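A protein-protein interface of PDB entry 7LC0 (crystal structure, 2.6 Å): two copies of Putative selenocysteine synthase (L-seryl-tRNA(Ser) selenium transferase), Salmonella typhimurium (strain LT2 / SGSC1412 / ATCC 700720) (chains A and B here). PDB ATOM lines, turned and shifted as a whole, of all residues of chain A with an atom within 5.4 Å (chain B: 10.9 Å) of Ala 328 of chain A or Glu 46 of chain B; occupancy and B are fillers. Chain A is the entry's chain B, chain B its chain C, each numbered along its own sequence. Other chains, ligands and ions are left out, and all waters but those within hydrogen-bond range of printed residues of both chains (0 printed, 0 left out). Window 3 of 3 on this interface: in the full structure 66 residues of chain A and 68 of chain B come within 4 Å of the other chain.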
ATOM      1  N   LEU A  11     -17.613   9.001   4.113  1.00  0.00           N
ATOM      2  CA  LEU A  11     -19.020   9.339   4.246  1.00  0.00           C
ATOM      3  C   LEU A  11     -19.513   9.026   5.652  1.00  0.00           C
ATOM      4  O   LEU A  11     -18.877   8.290   6.413  1.00  0.00           O
ATOM      5  CB  LEU A  11     -19.862   8.580   3.216  1.00  0.00           C
ATOM      6  CG  LEU A  11     -19.515   8.880   1.757  1.00  0.00           C
ATOM      7  CD1 LEU A  11     -20.368   8.047   0.819  1.00  0.00           C
ATOM      8  CD2 LEU A  11     -19.690  10.361   1.475  1.00  0.00           C
ATOM      9  N   LYS A  12     -20.663   9.600   5.992  1.00  0.00           N
ATOM     10  CA  LYS A  12     -21.252   9.376   7.300  1.00  0.00           C
ATOM     11  C   LYS A  12     -21.777   7.949   7.421  1.00  0.00           C
ATOM     12  O   LYS A  12     -22.078   7.279   6.429  1.00  0.00           O
ATOM     13  CB  LYS A  12     -22.392  10.361   7.557  1.00  0.00           C
ATOM     14  CG  LYS A  12     -21.972  11.814   7.688  1.00  0.00           C
ATOM     15  CD  LYS A  12     -23.155  12.674   8.109  1.00  0.00           C
ATOM     16  CE  LYS A  12     -22.762  14.134   8.278  1.00  0.00           C
ATOM     17  NZ  LYS A  12     -23.901  14.951   8.792  1.00  0.00           N
ATOM     18  N   LYS A  13     -21.885   7.484   8.663  1.00  0.00           N
ATOM     19  CA  LYS A  13     -22.568   6.230   8.950  1.00  0.00           C
ATOM     20  C   LYS A  13     -24.057   6.510   9.095  1.00  0.00           C
ATOM     21  O   LYS A  13     -24.459   7.354   9.904  1.00  0.00           O
ATOM     22  CB  LYS A  13     -22.013   5.587  10.217  1.00  0.00           C
ATOM     23  CG  LYS A  13     -22.734   4.310  10.619  1.00  0.00           C
ATOM     24  CD  LYS A  13     -22.173   3.732  11.906  1.00  0.00           C
ATOM     25  CE  LYS A  13     -22.906   2.460  12.301  1.00  0.00           C
ATOM     26  NZ  LYS A  13     -22.832   1.426  11.232  1.00  0.00           N
ATOM     27  N   VAL A  14     -24.873   5.819   8.309  1.00  0.00           N
ATOM     28  CA  VAL A  14     -26.309   6.065   8.254  1.00  0.00           C
ATOM     29  C   VAL A  14     -27.026   4.973   9.037  1.00  0.00           C
ATOM     30  O   VAL A  14     -26.904   3.784   8.718  1.00  0.00           O
ATOM     31  CB  VAL A  14     -26.812   6.124   6.804  1.00  0.00           C
ATOM     32  CG1 VAL A  14     -28.327   6.196   6.775  1.00  0.00           C
ATOM     33  CG2 VAL A  14     -26.203   7.318   6.088  1.00  0.00           C
ATOM     34  N   ILE A  15     -27.764   5.378  10.063  1.00  0.00           N
ATOM     35  CA  ILE A  15     -28.670   4.497  10.788  1.00  0.00           C
ATOM     36  C   ILE A  15     -30.076   4.807  10.294  1.00  0.00           C
ATOM     37  O   ILE A  15     -30.641   5.858  10.614  1.00  0.00           O
ATOM     38  CB  ILE A  15     -28.555   4.682  12.307  1.00  0.00           C
ATOM     39  CG1 ILE A  15     -27.169   4.252  12.792  1.00  0.00           C
ATOM     40  CG2 ILE A  15     -29.645   3.896  13.022  1.00  0.00           C
ATOM     41  CD1 ILE A  15     -26.998   4.329  14.296  1.00  0.00           C
ATOM     42  N   ASN A  16     -30.640   3.900   9.500  1.00  0.00           N
ATOM     43  CA  ASN A  16     -31.935   4.124   8.862  1.00  0.00           C
ATOM     44  C   ASN A  16     -33.035   3.622   9.789  1.00  0.00           C
ATOM     45  O   ASN A  16     -33.301   2.421   9.867  1.00  0.00           O
ATOM     46  CB  ASN A  16     -31.994   3.435   7.504  1.00  0.00           C
ATOM     47  CG  ASN A  16     -33.311   3.668   6.789  1.00  0.00           C
ATOM     48  OD1 ASN A  16     -34.068   4.577   7.132  1.00  0.00           O
ATOM     49  ND2 ASN A  16     -33.591   2.845   5.785  1.00  0.00           N
ATOM     50  N   ILE A  23     -33.378   8.098  -0.869  1.00  0.00           N
ATOM     51  CA  ILE A  23     -32.236   8.957  -0.574  1.00  0.00           C
ATOM     52  C   ILE A  23     -31.208   8.283   0.321  1.00  0.00           C
ATOM     53  O   ILE A  23     -30.095   8.800   0.467  1.00  0.00           O
ATOM     54  CB  ILE A  23     -32.695  10.277   0.079  1.00  0.00           C
ATOM     55  CG1 ILE A  23     -33.242  10.020   1.485  1.00  0.00           C
ATOM     56  CG2 ILE A  23     -33.747  10.960  -0.780  1.00  0.00           C
ATOM     57  CD1 ILE A  23     -33.682  11.275   2.206  1.00  0.00           C
ATOM     58  N   LEU A  24     -31.547   7.143   0.922  1.00  0.00           N
ATOM     59  CA  LEU A  24     -30.632   6.416   1.791  1.00  0.00           C
ATOM     60  C   LEU A  24     -30.152   5.108   1.174  1.00  0.00           C
ATOM     61  O   LEU A  24     -29.507   4.311   1.862  1.00  0.00           O
ATOM     62  CB  LEU A  24     -31.290   6.141   3.145  1.00  0.00           C
ATOM     63  CG  LEU A  24     -31.713   7.366   3.959  1.00  0.00           C
ATOM     64  CD1 LEU A  24     -32.244   6.942   5.318  1.00  0.00           C
ATOM     65  CD2 LEU A  24     -30.557   8.339   4.109  1.00  0.00           C
ATOM     66  N   LEU A 322     -30.121  14.457  15.113  1.00  0.00           N
ATOM     67  CA  LEU A 322     -29.970  13.041  14.788  1.00  0.00           C
ATOM     68  C   LEU A 322     -29.363  12.854  13.403  1.00  0.00           C
ATOM     69  O   LEU A 322     -28.561  11.937  13.190  1.00  0.00           O
ATOM     70  CB  LEU A 322     -31.320  12.333  14.886  1.00  0.00           C
ATOM     71  CG  LEU A 322     -31.861  12.121  16.301  1.00  0.00           C
ATOM     72  CD1 LEU A 322     -33.253  11.512  16.261  1.00  0.00           C
ATOM     73  CD2 LEU A 322     -30.914  11.242  17.098  1.00  0.00           C
ATOM     74  N   ARG A 323     -29.734  13.710  12.450  1.00  0.00           N
ATOM     75  CA  ARG A 323     -29.137  13.647  11.120  1.00  0.00           C
ATOM     76  C   ARG A 323     -27.828  14.420  11.045  1.00  0.00           C
ATOM     77  O   ARG A 323     -26.936  14.044  10.275  1.00  0.00           O
ATOM     78  CB  ARG A 323     -30.112  14.189  10.072  1.00  0.00           C
ATOM     79  CG  ARG A 323     -31.371  13.361   9.889  1.00  0.00           C
ATOM     80  CD  ARG A 323     -32.256  13.924   8.781  1.00  0.00           C
ATOM     81  NE  ARG A 323     -32.821  15.227   9.126  1.00  0.00           N
ATOM     82  CZ  ARG A 323     -32.340  16.390   8.697  1.00  0.00           C
ATOM     83  NH1 ARG A 323     -31.280  16.419   7.900  1.00  0.00           N
ATOM     84  NH2 ARG A 323     -32.920  17.525   9.063  1.00  0.00           N
ATOM     85  N   GLY A 325     -25.489  14.925  13.433  1.00  0.00           N
ATOM     86  CA  GLY A 325     -24.387  14.439  14.230  1.00  0.00           C
ATOM     87  C   GLY A 325     -23.382  13.659  13.399  1.00  0.00           C
ATOM     88  O   GLY A 325     -23.460  13.565  12.173  1.00  0.00           O
ATOM     89  N   GLU A 326     -22.403  13.090  14.106  1.00  0.00           N
ATOM     90  CA  GLU A 326     -21.391  12.273  13.442  1.00  0.00           C
ATOM     91  C   GLU A 326     -22.022  11.069  12.756  1.00  0.00           C
ATOM     92  O   GLU A 326     -21.588  10.667  11.670  1.00  0.00           O
ATOM     93  CB  GLU A 326     -20.332  11.826  14.450  1.00  0.00           C
ATOM     94  CG  GLU A 326     -19.492  12.964  15.002  1.00  0.00           C
ATOM     95  CD  GLU A 326     -18.472  12.494  16.017  1.00  0.00           C
ATOM     96  OE1 GLU A 326     -18.683  11.418  16.614  1.00  0.00           O
ATOM     97  OE2 GLU A 326     -17.460  13.198  16.215  1.00  0.00           O
ATOM     98  N   ILE A 327     -23.049  10.487  13.368  1.00  0.00           N
ATOM     99  CA  ILE A 327     -23.795   9.381  12.785  1.00  0.00           C
ATOM    100  C   ILE A 327     -25.128   9.923  12.294  1.00  0.00           C
ATOM    101  O   ILE A 327     -25.919  10.457  13.081  1.00  0.00           O
ATOM    102  CB  ILE A 327     -23.997   8.242  13.795  1.00  0.00           C
ATOM    103  CG1 ILE A 327     -22.649   7.652  14.212  1.00  0.00           C
ATOM    104  CG2 ILE A 327     -24.896   7.164  13.210  1.00  0.00           C
ATOM    105  CD1 ILE A 327     -22.760   6.529  15.220  1.00  0.00           C
ATOM    106  N   ALA A 328     -25.380   9.791  10.995  1.00  0.00           N
ATOM    107  CA  ALA A 328     -26.609  10.299  10.389  1.00  0.00           C
ATOM    108  C   ALA A 328     -27.749   9.347  10.722  1.00  0.00           C
ATOM    109  O   ALA A 328     -27.914   8.306  10.082  1.00  0.00           O
ATOM    110  CB  ALA A 328     -26.439  10.459   8.883  1.00  0.00           C
ATOM    111  N   ILE A 329     -28.541   9.704  11.727  1.00  0.00           N
ATOM    112  CA  ILE A 329     -29.701   8.922  12.139  1.00  0.00           C
ATOM    113  C   ILE A 329     -30.938   9.539  11.501  1.00  0.00           C
ATOM    114  O   ILE A 329     -31.263  10.704  11.760  1.00  0.00           O
ATOM    115  CB  ILE A 329     -29.832   8.873  13.668  1.00  0.00           C
ATOM    116  CG1 ILE A 329     -28.560   8.297  14.293  1.00  0.00           C
ATOM    117  CG2 ILE A 329     -31.047   8.052  14.070  1.00  0.00           C
ATOM    118  CD1 ILE A 329     -28.581   8.270  15.805  1.00  0.00           C
ATOM    119  N   TYR A 330     -31.624   8.763  10.668  1.00  0.00           N
ATOM    120  CA  TYR A 330     -32.814   9.219   9.960  1.00  0.00           C
ATOM    121  C   TYR A 330     -34.048   8.611  10.610  1.00  0.00           C
ATOM    122  O   TYR A 330     -34.157   7.384  10.715  1.00  0.00           O
ATOM    123  CB  TYR A 330     -32.745   8.844   8.479  1.00  0.00           C
ATOM    124  CG  TYR A 330     -31.789   9.701   7.684  1.00  0.00           C
ATOM    125  CD1 TYR A 330     -32.251  10.769   6.927  1.00  0.00           C
ATOM    126  CD2 TYR A 330     -30.424   9.449   7.698  1.00  0.00           C
ATOM    127  CE1 TYR A 330     -31.383  11.558   6.200  1.00  0.00           C
ATOM    128  CE2 TYR A 330     -29.546  10.234   6.975  1.00  0.00           C
ATOM    129  CZ  TYR A 330     -30.031  11.286   6.228  1.00  0.00           C
ATOM    130  OH  TYR A 330     -29.163  12.073   5.506  1.00  0.00           O
ATOM    131  N   ALA B  40     -21.304  -2.651   0.907  1.00  0.00           N
ATOM    132  CA  ALA B  40     -22.071  -1.488   0.480  1.00  0.00           C
ATOM    133  C   ALA B  40     -23.553  -1.810   0.350  1.00  0.00           C
ATOM    134  O   ALA B  40     -24.399  -0.942   0.594  1.00  0.00           O
ATOM    135  CB  ALA B  40     -21.526  -0.955  -0.843  1.00  0.00           C
ATOM    136  N   ALA B  43     -25.591  -1.794   3.933  1.00  0.00           N
ATOM    137  CA  ALA B  43     -25.623  -0.580   4.733  1.00  0.00           C
ATOM    138  C   ALA B  43     -26.248   0.546   3.925  1.00  0.00           C
ATOM    139  O   ALA B  43     -26.157   0.575   2.696  1.00  0.00           O
ATOM    140  CB  ALA B  43     -24.218  -0.171   5.196  1.00  0.00           C
ATOM    141  N   PHE B  44     -26.883   1.476   4.630  1.00  0.00           N
ATOM    142  CA  PHE B  44     -27.479   2.643   4.002  1.00  0.00           C
ATOM    143  C   PHE B  44     -26.470   3.785   3.936  1.00  0.00           C
ATOM    144  O   PHE B  44     -25.509   3.847   4.708  1.00  0.00           O
ATOM    145  CB  PHE B  44     -28.732   3.086   4.763  1.00  0.00           C
ATOM    146  CG  PHE B  44     -29.845   2.077   4.731  1.00  0.00           C
ATOM    147  CD1 PHE B  44     -29.942   1.103   5.710  1.00  0.00           C
ATOM    148  CD2 PHE B  44     -30.789   2.101   3.719  1.00  0.00           C
ATOM    149  CE1 PHE B  44     -30.964   0.172   5.683  1.00  0.00           C
ATOM    150  CE2 PHE B  44     -31.814   1.172   3.685  1.00  0.00           C
ATOM    151  CZ  PHE B  44     -31.902   0.207   4.668  1.00  0.00           C
ATOM    152  N   VAL B  45     -26.699   4.697   2.991  1.00  0.00           N
ATOM    153  CA  VAL B  45     -25.788   5.810   2.761  1.00  0.00           C
ATOM    154  C   VAL B  45     -26.568   6.930   2.089  1.00  0.00           C
ATOM    155  O   VAL B  45     -27.488   6.680   1.306  1.00  0.00           O
ATOM    156  CB  VAL B  45     -24.569   5.369   1.910  1.00  0.00           C
ATOM    157  CG1 VAL B  45     -25.016   4.932   0.521  1.00  0.00           C
ATOM    158  CG2 VAL B  45     -23.534   6.483   1.829  1.00  0.00           C
ATOM    159  N   GLU B  46     -26.201   8.169   2.406  1.00  0.00           N
ATOM    160  CA  GLU B  46     -26.774   9.330   1.732  1.00  0.00           C
ATOM    161  C   GLU B  46     -26.369   9.303   0.264  1.00  0.00           C
ATOM    162  O   GLU B  46     -25.203   9.539  -0.071  1.00  0.00           O
ATOM    163  CB  GLU B  46     -26.311  10.611   2.418  1.00  0.00           C
ATOM    164  CG  GLU B  46     -26.711  10.688   3.883  1.00  0.00           C
ATOM    165  CD  GLU B  46     -26.061  11.848   4.613  1.00  0.00           C
ATOM    166  OE1 GLU B  46     -25.077  12.408   4.087  1.00  0.00           O
ATOM    167  OE2 GLU B  46     -26.537  12.198   5.713  1.00  0.00           O
ATOM    168  N   ILE B  47     -27.333   9.012  -0.613  1.00  0.00           N
ATOM    169  CA  ILE B  47     -27.028   8.773  -2.023  1.00  0.00           C
ATOM    170  C   ILE B  47     -26.384   9.997  -2.659  1.00  0.00           C
ATOM    171  O   ILE B  47     -25.399   9.884  -3.397  1.00  0.00           O
ATOM    172  CB  ILE B  47     -28.301   8.343  -2.776  1.00  0.00           C
ATOM    173  CG1 ILE B  47     -28.691   6.919  -2.383  1.00  0.00           C
ATOM    174  CG2 ILE B  47     -28.094   8.434  -4.277  1.00  0.00           C
ATOM    175  CD1 ILE B  47     -27.657   5.880  -2.768  1.00  0.00           C
ATOM    176  N   ASP B  48     -26.925  11.188  -2.383  1.00  0.00           N
ATOM    177  CA  ASP B  48     -26.370  12.400  -2.979  1.00  0.00           C
ATOM    178  C   ASP B  48     -24.918  12.604  -2.563  1.00  0.00           C
ATOM    179  O   ASP B  48     -24.092  13.056  -3.365  1.00  0.00           O
ATOM    180  CB  ASP B  48     -27.222  13.612  -2.597  1.00  0.00           C
ATOM    181  CG  ASP B  48     -27.270  13.845  -1.101  1.00  0.00           C
ATOM    182  OD1 ASP B  48     -27.185  12.857  -0.342  1.00  0.00           O
ATOM    183  OD2 ASP B  48     -27.392  15.016  -0.686  1.00  0.00           O
ATOM    184  N   ALA B  49     -24.585  12.266  -1.315  1.00  0.00           N
ATOM    185  CA  ALA B  49     -23.195  12.337  -0.882  1.00  0.00           C
ATOM    186  C   ALA B  49     -22.356  11.238  -1.521  1.00  0.00           C
ATOM    187  O   ALA B  49     -21.167  11.444  -1.788  1.00  0.00           O
ATOM    188  CB  ALA B  49     -23.111  12.254   0.640  1.00  0.00           C
ATOM    189  N   LEU B  50     -22.954  10.072  -1.771  1.00  0.00           N
ATOM    190  CA  LEU B  50     -22.224   8.987  -2.418  1.00  0.00           C
ATOM    191  C   LEU B  50     -21.942   9.306  -3.881  1.00  0.00           C
ATOM    192  O   LEU B  50     -20.879   8.954  -4.405  1.00  0.00           O
ATOM    193  CB  LEU B  50     -23.011   7.681  -2.294  1.00  0.00           C
ATOM    194  CG  LEU B  50     -22.380   6.424  -2.898  1.00  0.00           C
ATOM    195  CD1 LEU B  50     -21.117   6.034  -2.145  1.00  0.00           C
ATOM    196  CD2 LEU B  50     -23.376   5.273  -2.912  1.00  0.00           C
ATOM    197  N   VAL B  51     -22.881   9.974  -4.556  1.00  0.00           N
ATOM    198  CA  VAL B  51     -22.677  10.339  -5.955  1.00  0.00           C
ATOM    199  C   VAL B  51     -21.512  11.311  -6.087  1.00  0.00           C
ATOM    200  O   VAL B  51     -20.724  11.237  -7.038  1.00  0.00           O
ATOM    201  CB  VAL B  51     -23.975  10.920  -6.549  1.00  0.00           C
ATOM    202  CG1 VAL B  51     -23.728  11.481  -7.940  1.00  0.00           C
ATOM    203  CG2 VAL B  51     -25.059   9.854  -6.596  1.00  0.00           C
ATOM    204  N   GLU B  52     -21.372  12.228  -5.126  1.00  0.00           N
ATOM    205  CA  GLU B  52     -20.273  13.185  -5.177  1.00  0.00           C
ATOM    206  C   GLU B  52     -18.938  12.516  -4.875  1.00  0.00           C
ATOM    207  O   GLU B  52     -17.930  12.808  -5.528  1.00  0.00           O
ATOM    208  CB  GLU B  52     -20.530  14.332  -4.200  1.00  0.00           C
ATOM    209  CG  GLU B  52     -21.771  15.147  -4.521  1.00  0.00           C
ATOM    210  CD  GLU B  52     -21.676  15.841  -5.864  1.00  0.00           C
ATOM    211  OE1 GLU B  52     -20.577  16.330  -6.204  1.00  0.00           O
ATOM    212  OE2 GLU B  52     -22.695  15.891  -6.584  1.00  0.00           O
ATOM    213  N   LYS B  53     -18.911  11.614  -3.891  1.00  0.00           N
ATOM    214  CA  LYS B  53     -17.655  10.980  -3.503  1.00  0.00           C
ATOM    215  C   LYS B  53     -17.163  10.023  -4.582  1.00  0.00           C
ATOM    216  O   LYS B  53     -15.977  10.022  -4.929  1.00  0.00           O
ATOM    217  CB  LYS B  53     -17.821  10.249  -2.171  1.00  0.00           C
ATOM    218  CG  LYS B  53     -17.150  10.943  -1.000  1.00  0.00           C
ATOM    219  CD  LYS B  53     -15.642  10.994  -1.176  1.00  0.00           C
ATOM    220  CE  LYS B  53     -14.976  11.691   0.000  1.00  0.00           C
ATOM    221  NZ  LYS B  53     -13.491  11.704  -0.129  1.00  0.00           N
ATOM    222  N   THR B  54     -18.062   9.196  -5.121  1.00  0.00           N
ATOM    223  CA  THR B  54     -17.655   8.251  -6.156  1.00  0.00           C
ATOM    224  C   THR B  54     -17.199   8.977  -7.416  1.00  0.00           C
ATOM    225  O   THR B  54     -16.262   8.534  -8.091  1.00  0.00           O
ATOM    226  CB  THR B  54     -18.797   7.284  -6.470  1.00  0.00           C
ATOM    227  OG1 THR B  54     -19.975   8.023  -6.816  1.00  0.00           O
ATOM    228  CG2 THR B  54     -19.089   6.399  -5.266  1.00  0.00           C
ATOM    229  N   GLY B  55     -17.840  10.099  -7.745  1.00  0.00           N
ATOM    230  CA  GLY B  55     -17.376  10.892  -8.870  1.00  0.00           C
ATOM    231  C   GLY B  55     -15.990  11.460  -8.641  1.00  0.00           C
ATOM    232  O   GLY B  55     -15.186  11.563  -9.570  1.00  0.00           O
ATOM    233  N   GLY B 247     -27.098   0.893  -8.346  1.00  0.00           N
ATOM    234  CA  GLY B 247     -27.281   1.040  -6.920  1.00  0.00           C
ATOM    235  C   GLY B 247     -25.990   1.336  -6.185  1.00  0.00           C
ATOM    236  O   GLY B 247     -24.916   1.472  -6.768  1.00  0.00           O
ATOM    237  N   LYS B 248     -26.118   1.428  -4.860  1.00  0.00           N
ATOM    238  CA  LYS B 248     -24.977   1.764  -4.017  1.00  0.00           C
ATOM    239  C   LYS B 248     -23.923   0.663  -4.018  1.00  0.00           C
ATOM    240  O   LYS B 248     -22.741   0.944  -3.788  1.00  0.00           O
ATOM    241  CB  LYS B 248     -25.457   2.041  -2.591  1.00  0.00           C
ATOM    242  CG  LYS B 248     -26.102   0.840  -1.918  1.00  0.00           C
ATOM    243  CD  LYS B 248     -27.018   1.256  -0.780  1.00  0.00           C
ATOM    244  CE  LYS B 248     -27.569   0.036  -0.055  1.00  0.00           C
ATOM    245  NZ  LYS B 248     -28.093  -0.994  -0.997  1.00  0.00           N
ATOM    246  N   MET B 251     -21.773   1.023  -7.405  1.00  0.00           N
ATOM    247  CA  MET B 251     -21.032   2.277  -7.426  1.00  0.00           C
ATOM    248  C   MET B 251     -19.766   2.125  -6.594  1.00  0.00           C
ATOM    249  O   MET B 251     -18.684   2.551  -7.000  1.00  0.00           O
ATOM    250  CB  MET B 251     -21.891   3.424  -6.898  1.00  0.00           C
ATOM    251  CG  MET B 251     -23.029   3.814  -7.817  1.00  0.00           C
ATOM    252  SD  MET B 251     -24.268   5.041  -6.958  1.00  0.00           S
ATOM    253  CE  MET B 251     -23.026   6.484  -6.544  1.00  0.00           C
ATOM    254  N   VAL B 252     -19.916   1.506  -5.421  1.00  0.00           N
ATOM    255  CA  VAL B 252     -18.760   1.210  -4.584  1.00  0.00           C
ATOM    256  C   VAL B 252     -17.904   0.127  -5.230  1.00  0.00           C
ATOM    257  O   VAL B 252     -16.670   0.166  -5.158  1.00  0.00           O
ATOM    258  CB  VAL B 252     -19.217   0.811  -3.168  1.00  0.00           C
ATOM    259  CG1 VAL B 252     -18.038   0.339  -2.327  1.00  0.00           C
ATOM    260  CG2 VAL B 252     -19.918   1.980  -2.493  1.00  0.00           C
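O of Leu 24 of chain A is in hydrogen-bond range of N of Val 45 of chain B, at 3.1 Å. OH of Tyr 330 of chain A sits at hydrogen-bond distance from OE2 of Glu 46 of chain B. The backbone carbonyl oxygen (O) of Val 45 of chain B lies close to the backbone carbonyl oxygen (O) of Ile 23 of chain A (3.5 Å). N of Ile 47 of chain B lies within hydrogen-bond range of O of Ile 23 of chain A, at 3.0 Å.
The side-chain hydroxyl of Thr 54 of chain B lies within hydrogen-bond range of the backbone carbonyl oxygen of Leu 50 of chain B (2.7 Å). O of Lys 13 of chain A is in hydrogen-bond range of N of Ala 328 of chain A. N of Ile 15 of chain A lies within hydrogen-bond range of O of Ala 328 of chain A, at 2.9 Å. N of Tyr 330 of chain A is in hydrogen-bond range of O of Ile 15 of chain A.
Among the printed residues, pairs that only touch across the chains: Leu 11 of chain A with Val 45 of chain B (3.7 Å), Leu 11 of chain A with Ala 49 of chain B (3.7 Å), Leu 11 of chain A with Leu 50 of chain B (3.7 Å), Leu 11 of chain A with Lys 53 of chain B (3.6 Å), Val 14 of chain A with Phe 44 of chain B (3.4 Å), Val 14 of chain A with Val 45 of chain B (3.7 Å), Val 14 of chain A with Glu 46 of chain B (3.8 Å), Asn 16 of chain A with Phe 44 of chain B (3.2 Å), Ile 23 of chain A with Glu 46 of chain B (3.6 Å), Leu 24 of chain A with Phe 44 of chain B (3.2 Å) and Ala 328 of chain A with Glu 46 of chain B (3.6 Å).
No residue of chain B comes within 4 Å of Lys 12 of chain A. Val 14 of chain A touches just these residues of chain B: Phe 44, Val 45 and Glu 46. Ile 15 of chain A touches none of the printed residues of chain B. Printed residues of chain B within 4 Å of Asn 16 of chain A: Phe 44. Printed residues of chain B within 4 Å of Ile 23 of chain A: Val 45 (3.5 Å), Glu 46 (3.6 Å) and Ile 47 (3.0 Å). Arg 323 of chain A touches none of the printed residues of chain B. No residue of chain B comes within 4 Å of Gly 325 of chain A. No residue of chain B comes within 4 Å of Ile 327 of chain A. Of chain B, only Glu 46 comes within 4 Å of Tyr 330 of chain A. Glu 46 of chain B touches four residues of chain A. Glu 52 of chain B touches none of the printed residues of chain A. The nearest residue of chain B that does not touch Ala 328 of chain A is Phe 44 of chain B (7.4 Å).
Of the 16 printed residues of chain A, 7 touch a printed residue of chain B. Hydrophobic or aromatic side chains of chain A within 4 Å of the printed part of chain B: Leu 11, Val 14, Ala 328 and Tyr 330. Printed residues of chain B that touch a printed residue of chain A: Phe 44, Val 45, Glu 46, Ile 47, Ala 49, Leu 50 and Lys 53. Hydrophobic or aromatic side chains of chain B within 4 Å of the printed part of chain A: Phe 44, Val 45, Ile 47, Ala 49 and Leu 50. Among the printed residues, no Asp or Glu carboxylate lies within 4 Å of a Lys or Arg side-chain nitrogen of the other chain.
No position is printed for both chains.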
